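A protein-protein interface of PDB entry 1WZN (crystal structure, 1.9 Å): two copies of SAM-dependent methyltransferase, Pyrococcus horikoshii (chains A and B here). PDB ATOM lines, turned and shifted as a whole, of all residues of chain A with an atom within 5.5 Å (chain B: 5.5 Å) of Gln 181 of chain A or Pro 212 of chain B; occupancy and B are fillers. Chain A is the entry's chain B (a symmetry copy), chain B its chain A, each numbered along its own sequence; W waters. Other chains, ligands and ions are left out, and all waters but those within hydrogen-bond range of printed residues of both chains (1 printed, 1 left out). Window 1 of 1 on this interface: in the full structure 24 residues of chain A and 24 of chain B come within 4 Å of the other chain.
OE1 of Gln 181 of chain A sits close to OG1 of Thr 211 of chain B, 3.4 Å away. OG1 of Thr 211 of chain B lies within hydrogen-bond range of OE2 of Glu 214 of chain A (3.0 Å). N of Arg 213 of chain B lies within hydrogen-bond range of OE1 of Gln 181 of chain A. The side-chain carboxylate of Glu 214 of chain A lies within salt-bridge range of the guanidinium group of Arg 213 of chain B. OH of Tyr 243 of chain B is in hydrogen-bond range of N of Ala 179 of chain A.
The backbone NH (N) of Tyr 243 of chain B lies within hydrogen-bond range of the backbone carbonyl oxygen (O) of Phe 145 of chain B (2.8 Å). The side-chain amide nitrogen of Gln 181 of chain A is in hydrogen-bond range of the backbone carbonyl oxygen of Ile 209 of chain A (2.8 Å). The backbone NH (N) of Thr 211 of chain B lies within hydrogen-bond range of the side-chain carboxylate (OE2) of Glu 214 of chain B (2.8 Å). The side-chain amide nitrogen (NE2) of Gln 181 of chain A sits at hydrogen-bond distance from the side-chain carboxylate (OE1) of Glu 214 of chain A, at 3.0 Å.
C of Pro 178 of chain A touches OH of Tyr 243 of chain B, at 3.7 Å. Val 180 of chain A touches Arg 213 of chain B (O to NH2, 3.7 Å). CD of Pro 212 of chain B touches OE1 of Gln 181 of chain A (3.5 Å). Arg 213 of chain B touches Tyr 210 of chain A (NH1 to CE1, 3.3 Å). Glu 214 of chain B touches Glu 214 of chain A.
Printed residues of chain A within 4 Å of Pro 212 of chain B: Gln 181 (3.5 Å). Printed residues of chain A within 4 Å of Thr 211 of chain B: Gln 181 and Glu 214. Of the printed residues of chain B, Val 180 of chain A touches Arg 213 (3.7 Å). Printed residues of chain B within 4 Å of Pro 178 of chain A: Tyr 243 (3.7 Å). Of the printed residues of chain A, Tyr 243 of chain B touches Pro 178 and Ala 179. The nearest residue of chain B that does not touch Gln 181 of chain A is Glu 214 of chain B (4.7 Å).
Of the 12 printed residues of chain B, 5 touch a printed residue of chain A. Hydrophobic or aromatic side chains of chain B that line the printed part of chain A: Pro 212 and Tyr 243. Of the 12 printed residues of chain A, 6 touch a printed residue of chain B. Hydrophobic or aromatic side chains of chain A within 4 Å of the printed part of chain B: Pro 178, Ala 179 and Tyr 210. Among the printed residues, 10 pairs touch across the chains. Among the printed residues, Asp or Glu carboxylates within 4 Å of a Lys or Arg side-chain nitrogen of the other chain: Glu 214 of chain A with Arg 213 of chain B (3.7 Å).
Glu 214 of chain B touches its own counterpart, Glu 214 of chain A. Positions printed for both chains: 210 and 214.
Water W1 lies within hydrogen-bond range of O of Val 180 of chain A (2.8 Å) and NH2 of Arg 213 of chain B (3.5 Å).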
ATOM      1  N   GLU A 177       5.250  34.582  -0.893  1.00  0.00           N
ATOM      2  CA  GLU A 177       5.227  34.740  -2.345  1.00  0.00           C
ATOM      3  C   GLU A 177       5.307  33.297  -2.829  1.00  0.00           C
ATOM      4  O   GLU A 177       6.384  32.782  -3.120  1.00  0.00           O
ATOM      5  CB  GLU A 177       6.444  35.533  -2.824  1.00  0.00           C
ATOM      6  CG  GLU A 177       6.502  36.963  -2.303  1.00  0.00           C
ATOM      7  CD  GLU A 177       7.646  37.749  -2.909  1.00  0.00           C
ATOM      8  OE1 GLU A 177       8.799  37.285  -2.826  1.00  0.00           O
ATOM      9  OE2 GLU A 177       7.393  38.835  -3.473  1.00  0.00           O
ATOM     10  N   PRO A 178       4.153  32.624  -2.905  1.00  0.00           N
ATOM     11  CA  PRO A 178       4.011  31.228  -3.327  1.00  0.00           C
ATOM     12  C   PRO A 178       4.628  30.844  -4.661  1.00  0.00           C
ATOM     13  O   PRO A 178       5.261  29.794  -4.774  1.00  0.00           O
ATOM     14  CB  PRO A 178       2.498  31.017  -3.301  1.00  0.00           C
ATOM     15  CG  PRO A 178       1.977  32.362  -3.683  1.00  0.00           C
ATOM     16  CD  PRO A 178       2.835  33.284  -2.846  1.00  0.00           C
ATOM     17  N   ALA A 179       4.448  31.693  -5.667  1.00  0.00           N
ATOM     18  CA  ALA A 179       4.973  31.419  -7.000  1.00  0.00           C
ATOM     19  C   ALA A 179       6.471  31.150  -7.008  1.00  0.00           C
ATOM     20  O   ALA A 179       6.933  30.201  -7.649  1.00  0.00           O
ATOM     21  CB  ALA A 179       4.652  32.574  -7.929  1.00  0.00           C
ATOM     22  N   VAL A 180       7.226  31.991  -6.302  1.00  0.00           N
ATOM     23  CA  VAL A 180       8.674  31.856  -6.238  1.00  0.00           C
ATOM     24  C   VAL A 180       9.142  31.166  -4.959  1.00  0.00           C
ATOM     25  O   VAL A 180      10.338  31.130  -4.664  1.00  0.00           O
ATOM     26  CB  VAL A 180       9.370  33.236  -6.354  1.00  0.00           C
ATOM     27  CG1 VAL A 180       9.194  33.788  -7.768  1.00  0.00           C
ATOM     28  CG2 VAL A 180       8.788  34.214  -5.330  1.00  0.00           C
ATOM     29  N   GLN A 181       8.190  30.616  -4.210  1.00  0.00           N
ATOM     30  CA  GLN A 181       8.483  29.912  -2.967  1.00  0.00           C
ATOM     31  C   GLN A 181       9.384  30.711  -2.035  1.00  0.00           C
ATOM     32  O   GLN A 181      10.391  30.204  -1.528  1.00  0.00           O
ATOM     33  CB  GLN A 181       9.105  28.551  -3.285  1.00  0.00           C
ATOM     34  CG  GLN A 181       8.125  27.642  -4.011  1.00  0.00           C
ATOM     35  CD  GLN A 181       8.752  26.372  -4.535  1.00  0.00           C
ATOM     36  OE1 GLN A 181       8.572  26.022  -5.701  1.00  0.00           O
ATOM     37  NE2 GLN A 181       9.487  25.666  -3.677  1.00  0.00           N
ATOM     38  N   LYS A 182       9.011  31.969  -1.820  1.00  0.00           N
ATOM     39  CA  LYS A 182       9.758  32.860  -0.939  1.00  0.00           C
ATOM     40  C   LYS A 182       8.864  33.261   0.220  1.00  0.00           C
ATOM     41  O   LYS A 182       7.649  33.396   0.068  1.00  0.00           O
ATOM     42  CB  LYS A 182      10.203  34.122  -1.677  1.00  0.00           C
ATOM     43  CG  LYS A 182      11.270  33.910  -2.738  1.00  0.00           C
ATOM     44  CD  LYS A 182      12.615  33.574  -2.123  1.00  0.00           C
ATOM     45  CE  LYS A 182      13.709  33.533  -3.193  1.00  0.00           C
ATOM     46  NZ  LYS A 182      15.059  33.272  -2.616  1.00  0.00           N
ATOM     47  N   LEU A 183       9.477  33.458   1.377  1.00  0.00           N
ATOM     48  CA  LEU A 183       8.739  33.842   2.563  1.00  0.00           C
ATOM     49  C   LEU A 183       9.530  34.931   3.269  1.00  0.00           C
ATOM     50  O   LEU A 183      10.753  34.837   3.408  1.00  0.00           O
ATOM     51  CB  LEU A 183       8.553  32.622   3.472  1.00  0.00           C
ATOM     52  CG  LEU A 183       7.745  32.791   4.758  1.00  0.00           C
ATOM     53  CD1 LEU A 183       7.093  31.465   5.119  1.00  0.00           C
ATOM     54  CD2 LEU A 183       8.646  33.280   5.877  1.00  0.00           C
ATOM     55  N   LEU A 207      13.286  34.033   3.343  1.00  0.00           N
ATOM     56  CA  LEU A 207      13.454  32.589   3.456  1.00  0.00           C
ATOM     57  C   LEU A 207      12.899  31.876   2.232  1.00  0.00           C
ATOM     58  O   LEU A 207      12.142  32.454   1.450  1.00  0.00           O
ATOM     59  CB  LEU A 207      12.767  32.062   4.718  1.00  0.00           C
ATOM     60  CG  LEU A 207      13.297  32.634   6.041  1.00  0.00           C
ATOM     61  CD1 LEU A 207      12.573  31.973   7.203  1.00  0.00           C
ATOM     62  CD2 LEU A 207      14.796  32.393   6.148  1.00  0.00           C
ATOM     63  N   ASN A 208      13.288  30.617   2.078  1.00  0.00           N
ATOM     64  CA  ASN A 208      12.864  29.809   0.946  1.00  0.00           C
ATOM     65  C   ASN A 208      11.976  28.682   1.434  1.00  0.00           C
ATOM     66  O   ASN A 208      12.243  28.074   2.474  1.00  0.00           O
ATOM     67  CB  ASN A 208      14.098  29.252   0.229  1.00  0.00           C
ATOM     68  CG  ASN A 208      14.985  30.347  -0.323  1.00  0.00           C
ATOM     69  OD1 ASN A 208      14.792  30.810  -1.446  1.00  0.00           O
ATOM     70  ND2 ASN A 208      15.954  30.785   0.474  1.00  0.00           N
ATOM     71  N   ILE A 209      10.922  28.410   0.673  1.00  0.00           N
ATOM     72  CA  ILE A 209       9.958  27.374   1.015  1.00  0.00           C
ATOM     73  C   ILE A 209      10.185  26.087   0.230  1.00  0.00           C
ATOM     74  O   ILE A 209      10.160  26.092  -1.000  1.00  0.00           O
ATOM     75  CB  ILE A 209       8.521  27.855   0.739  1.00  0.00           C
ATOM     76  CG1 ILE A 209       8.252  29.155   1.505  1.00  0.00           C
ATOM     77  CG2 ILE A 209       7.529  26.774   1.144  1.00  0.00           C
ATOM     78  CD1 ILE A 209       6.912  29.789   1.193  1.00  0.00           C
ATOM     79  N   TYR A 210      10.398  24.990   0.955  1.00  0.00           N
ATOM     80  CA  TYR A 210      10.625  23.679   0.346  1.00  0.00           C
ATOM     81  C   TYR A 210       9.697  22.638   0.947  1.00  0.00           C
ATOM     82  O   TYR A 210       9.312  22.737   2.109  1.00  0.00           O
ATOM     83  CB  TYR A 210      12.052  23.192   0.609  1.00  0.00           C
ATOM     84  CG  TYR A 210      13.150  24.012  -0.007  1.00  0.00           C
ATOM     85  CD1 TYR A 210      13.446  23.913  -1.369  1.00  0.00           C
ATOM     86  CD2 TYR A 210      13.911  24.878   0.775  1.00  0.00           C
ATOM     87  CE1 TYR A 210      14.475  24.654  -1.930  1.00  0.00           C
ATOM     88  CE2 TYR A 210      14.939  25.623   0.225  1.00  0.00           C
ATOM     89  CZ  TYR A 210      15.219  25.509  -1.125  1.00  0.00           C
ATOM     90  OH  TYR A 210      16.239  26.261  -1.660  1.00  0.00           O
ATOM     91  N   GLU A 214      10.805  17.882  -2.281  1.00  0.00           N
ATOM     92  CA  GLU A 214      11.694  18.803  -2.966  1.00  0.00           C
ATOM     93  C   GLU A 214      13.122  18.730  -2.432  1.00  0.00           C
ATOM     94  O   GLU A 214      14.085  18.718  -3.208  1.00  0.00           O
ATOM     95  CB  GLU A 214      11.143  20.219  -2.828  1.00  0.00           C
ATOM     96  CG  GLU A 214      11.672  21.205  -3.832  1.00  0.00           C
ATOM     97  CD  GLU A 214      10.870  22.489  -3.833  1.00  0.00           C
ATOM     98  OE1 GLU A 214      11.305  23.457  -4.487  1.00  0.00           O
ATOM     99  OE2 GLU A 214       9.802  22.528  -3.184  1.00  0.00           O
ATOM    100  N   PHE B 145      -1.252  23.815 -13.308  1.00  0.00           N
ATOM    101  CA  PHE B 145      -1.679  23.329 -12.005  1.00  0.00           C
ATOM    102  C   PHE B 145      -1.747  24.516 -11.056  1.00  0.00           C
ATOM    103  O   PHE B 145      -1.090  25.535 -11.272  1.00  0.00           O
ATOM    104  CB  PHE B 145      -0.739  22.226 -11.496  1.00  0.00           C
ATOM    105  CG  PHE B 145       0.692  22.642 -11.388  1.00  0.00           C
ATOM    106  CD1 PHE B 145       1.260  22.901 -10.146  1.00  0.00           C
ATOM    107  CD2 PHE B 145       1.477  22.771 -12.525  1.00  0.00           C
ATOM    108  CE1 PHE B 145       2.596  23.282 -10.040  1.00  0.00           C
ATOM    109  CE2 PHE B 145       2.808  23.150 -12.431  1.00  0.00           C
ATOM    110  CZ  PHE B 145       3.370  23.406 -11.185  1.00  0.00           C
ATOM    111  N   TYR B 210       2.180  19.505  -5.296  1.00  0.00           N
ATOM    112  CA  TYR B 210       3.496  19.810  -5.848  1.00  0.00           C
ATOM    113  C   TYR B 210       3.736  21.313  -5.910  1.00  0.00           C
ATOM    114  O   TYR B 210       2.801  22.085  -6.123  1.00  0.00           O
ATOM    115  CB  TYR B 210       3.610  19.279  -7.279  1.00  0.00           C
ATOM    116  CG  TYR B 210       3.561  17.780  -7.433  1.00  0.00           C
ATOM    117  CD1 TYR B 210       4.655  16.988  -7.093  1.00  0.00           C
ATOM    118  CD2 TYR B 210       2.432  17.155  -7.963  1.00  0.00           C
ATOM    119  CE1 TYR B 210       4.632  15.610  -7.285  1.00  0.00           C
ATOM    120  CE2 TYR B 210       2.395  15.780  -8.155  1.00  0.00           C
ATOM    121  CZ  TYR B 210       3.501  15.015  -7.814  1.00  0.00           C
ATOM    122  OH  TYR B 210       3.462  13.654  -7.993  1.00  0.00           O
ATOM    123  N   THR B 211       4.989  21.721  -5.741  1.00  0.00           N
ATOM    124  CA  THR B 211       5.342  23.131  -5.844  1.00  0.00           C
ATOM    125  C   THR B 211       5.859  23.304  -7.265  1.00  0.00           C
ATOM    126  O   THR B 211       6.165  22.319  -7.938  1.00  0.00           O
ATOM    127  CB  THR B 211       6.470  23.518  -4.886  1.00  0.00           C
ATOM    128  OG1 THR B 211       7.642  22.754  -5.203  1.00  0.00           O
ATOM    129  CG2 THR B 211       6.050  23.261  -3.436  1.00  0.00           C
ATOM    130  N   PRO B 212       5.957  24.549  -7.742  1.00  0.00           N
ATOM    131  CA  PRO B 212       6.453  24.777  -9.103  1.00  0.00           C
ATOM    132  C   PRO B 212       7.870  24.234  -9.274  1.00  0.00           C
ATOM    133  O   PRO B 212       8.194  23.623 -10.291  1.00  0.00           O
ATOM    134  CB  PRO B 212       6.396  26.294  -9.236  1.00  0.00           C
ATOM    135  CG  PRO B 212       5.206  26.643  -8.401  1.00  0.00           C
ATOM    136  CD  PRO B 212       5.408  25.792  -7.172  1.00  0.00           C
ATOM    137  N   ARG B 213       8.709  24.453  -8.268  1.00  0.00           N
ATOM    138  CA  ARG B 213      10.086  23.981  -8.330  1.00  0.00           C
ATOM    139  C   ARG B 213      10.151  22.458  -8.394  1.00  0.00           C
ATOM    140  O   ARG B 213      11.002  21.899  -9.086  1.00  0.00           O
ATOM    141  CB  ARG B 213      10.874  24.498  -7.127  1.00  0.00           C
ATOM    142  CG  ARG B 213      12.355  24.140  -7.152  1.00  0.00           C
ATOM    143  CD  ARG B 213      13.082  24.891  -6.053  1.00  0.00           C
ATOM    144  NE  ARG B 213      12.940  26.331  -6.237  1.00  0.00           N
ATOM    145  CZ  ARG B 213      12.911  27.216  -5.245  1.00  0.00           C
ATOM    146  NH1 ARG B 213      13.014  26.813  -3.985  1.00  0.00           N
ATOM    147  NH2 ARG B 213      12.771  28.504  -5.518  1.00  0.00           N
ATOM    148  N   GLU B 214       9.254  21.789  -7.675  1.00  0.00           N
ATOM    149  CA  GLU B 214       9.210  20.328  -7.678  1.00  0.00           C
ATOM    150  C   GLU B 214       8.931  19.804  -9.077  1.00  0.00           C
ATOM    151  O   GLU B 214       9.610  18.903  -9.566  1.00  0.00           O
ATOM    152  CB  GLU B 214       8.102  19.811  -6.768  1.00  0.00           C
ATOM    153  CG  GLU B 214       8.421  19.750  -5.305  1.00  0.00           C
ATOM    154  CD  GLU B 214       7.224  19.279  -4.515  1.00  0.00           C
ATOM    155  OE1 GLU B 214       7.383  18.906  -3.347  1.00  0.00           O
ATOM    156  OE2 GLU B 214       6.110  19.282  -5.069  1.00  0.00           O
ATOM    157  N   VAL B 215       7.905  20.358  -9.710  1.00  0.00           N
ATOM    158  CA  VAL B 215       7.553  19.923 -11.052  1.00  0.00           C
ATOM    159  C   VAL B 215       8.710  20.170 -12.015  1.00  0.00           C
ATOM    160  O   VAL B 215       9.015  19.315 -12.846  1.00  0.00           O
ATOM    161  CB  VAL B 215       6.290  20.640 -11.558  1.00  0.00           C
ATOM    162  CG1 VAL B 215       5.899  20.090 -12.933  1.00  0.00           C
ATOM    163  CG2 VAL B 215       5.145  20.420 -10.571  1.00  0.00           C
ATOM    164  N   ARG B 216       9.361  21.325 -11.901  1.00  0.00           N
ATOM    165  CA  ARG B 216      10.489  21.631 -12.776  1.00  0.00           C
ATOM    166  C   ARG B 216      11.617  20.618 -12.590  1.00  0.00           C
ATOM    167  O   ARG B 216      12.180  20.119 -13.568  1.00  0.00           O
ATOM    168  CB  ARG B 216      11.017  23.049 -12.528  1.00  0.00           C
ATOM    169  CG  ARG B 216      12.305  23.344 -13.293  1.00  0.00           C
ATOM    170  CD  ARG B 216      12.710  24.812 -13.261  1.00  0.00           C
ATOM    171  NE  ARG B 216      12.992  25.299 -11.914  1.00  0.00           N
ATOM    172  CZ  ARG B 216      13.919  24.794 -11.107  1.00  0.00           C
ATOM    173  NH1 ARG B 216      14.671  23.775 -11.499  1.00  0.00           N
ATOM    174  NH2 ARG B 216      14.094  25.315  -9.902  1.00  0.00           N
ATOM    175  N   LEU B 217      11.942  20.307 -11.337  1.00  0.00           N
ATOM    176  CA  LEU B 217      12.999  19.342 -11.036  1.00  0.00           C
ATOM    177  C   LEU B 217      12.662  17.965 -11.596  1.00  0.00           C
ATOM    178  O   LEU B 217      13.542  17.238 -12.060  1.00  0.00           O
ATOM    179  CB  LEU B 217      13.208  19.223  -9.522  1.00  0.00           C
ATOM    180  CG  LEU B 217      13.796  20.425  -8.783  1.00  0.00           C
ATOM    181  CD1 LEU B 217      13.744  20.161  -7.284  1.00  0.00           C
ATOM    182  CD2 LEU B 217      15.233  20.668  -9.243  1.00  0.00           C
ATOM    183  N   ILE B 228       8.774  27.730 -16.208  1.00  0.00           N
ATOM    184  CA  ILE B 228       7.653  27.830 -15.284  1.00  0.00           C
ATOM    185  C   ILE B 228       7.066  29.212 -15.499  1.00  0.00           C
ATOM    186  O   ILE B 228       7.763  30.216 -15.340  1.00  0.00           O
ATOM    187  CB  ILE B 228       8.113  27.701 -13.811  1.00  0.00           C
ATOM    188  CG1 ILE B 228       8.828  26.366 -13.604  1.00  0.00           C
ATOM    189  CG2 ILE B 228       6.907  27.795 -12.874  1.00  0.00           C
ATOM    190  CD1 ILE B 228       9.387  26.179 -12.203  1.00  0.00           C
ATOM    191  N   TYR B 243       0.051  27.931 -12.133  1.00  0.00           N
ATOM    192  CA  TYR B 243       1.311  27.766 -12.836  1.00  0.00           C
ATOM    193  C   TYR B 243       1.226  26.925 -14.090  1.00  0.00           C
ATOM    194  O   TYR B 243       0.330  26.094 -14.241  1.00  0.00           O
ATOM    195  CB  TYR B 243       2.330  27.142 -11.884  1.00  0.00           C
ATOM    196  CG  TYR B 243       2.310  27.811 -10.532  1.00  0.00           C
ATOM    197  CD1 TYR B 243       2.696  29.138 -10.394  1.00  0.00           C
ATOM    198  CD2 TYR B 243       1.816  27.143  -9.413  1.00  0.00           C
ATOM    199  CE1 TYR B 243       2.585  29.801  -9.170  1.00  0.00           C
ATOM    200  CE2 TYR B 243       1.699  27.794  -8.180  1.00  0.00           C
ATOM    201  CZ  TYR B 243       2.081  29.125  -8.073  1.00  0.00           C
ATOM    202  OH  TYR B 243       1.925  29.792  -6.879  1.00  0.00           O
ATOM    203  N   ILE B 245       3.843  24.621 -16.593  1.00  0.00           N
ATOM    204  CA  ILE B 245       5.154  24.035 -16.792  1.00  0.00           C
ATOM    205  C   ILE B 245       5.236  23.770 -18.291  1.00  0.00           C
ATOM    206  O   ILE B 245       4.327  23.179 -18.874  1.00  0.00           O
ATOM    207  CB  ILE B 245       5.319  22.704 -16.033  1.00  0.00           C
ATOM    208  CG1 ILE B 245       5.321  22.960 -14.521  1.00  0.00           C
ATOM    209  CG2 ILE B 245       6.616  22.025 -16.453  1.00  0.00           C
ATOM    210  CD1 ILE B 245       6.469  23.821 -14.038  1.00  0.00           C
HETATM  211  O   HOH W   1      12.340  31.816  -6.532  1.00  0.00           O
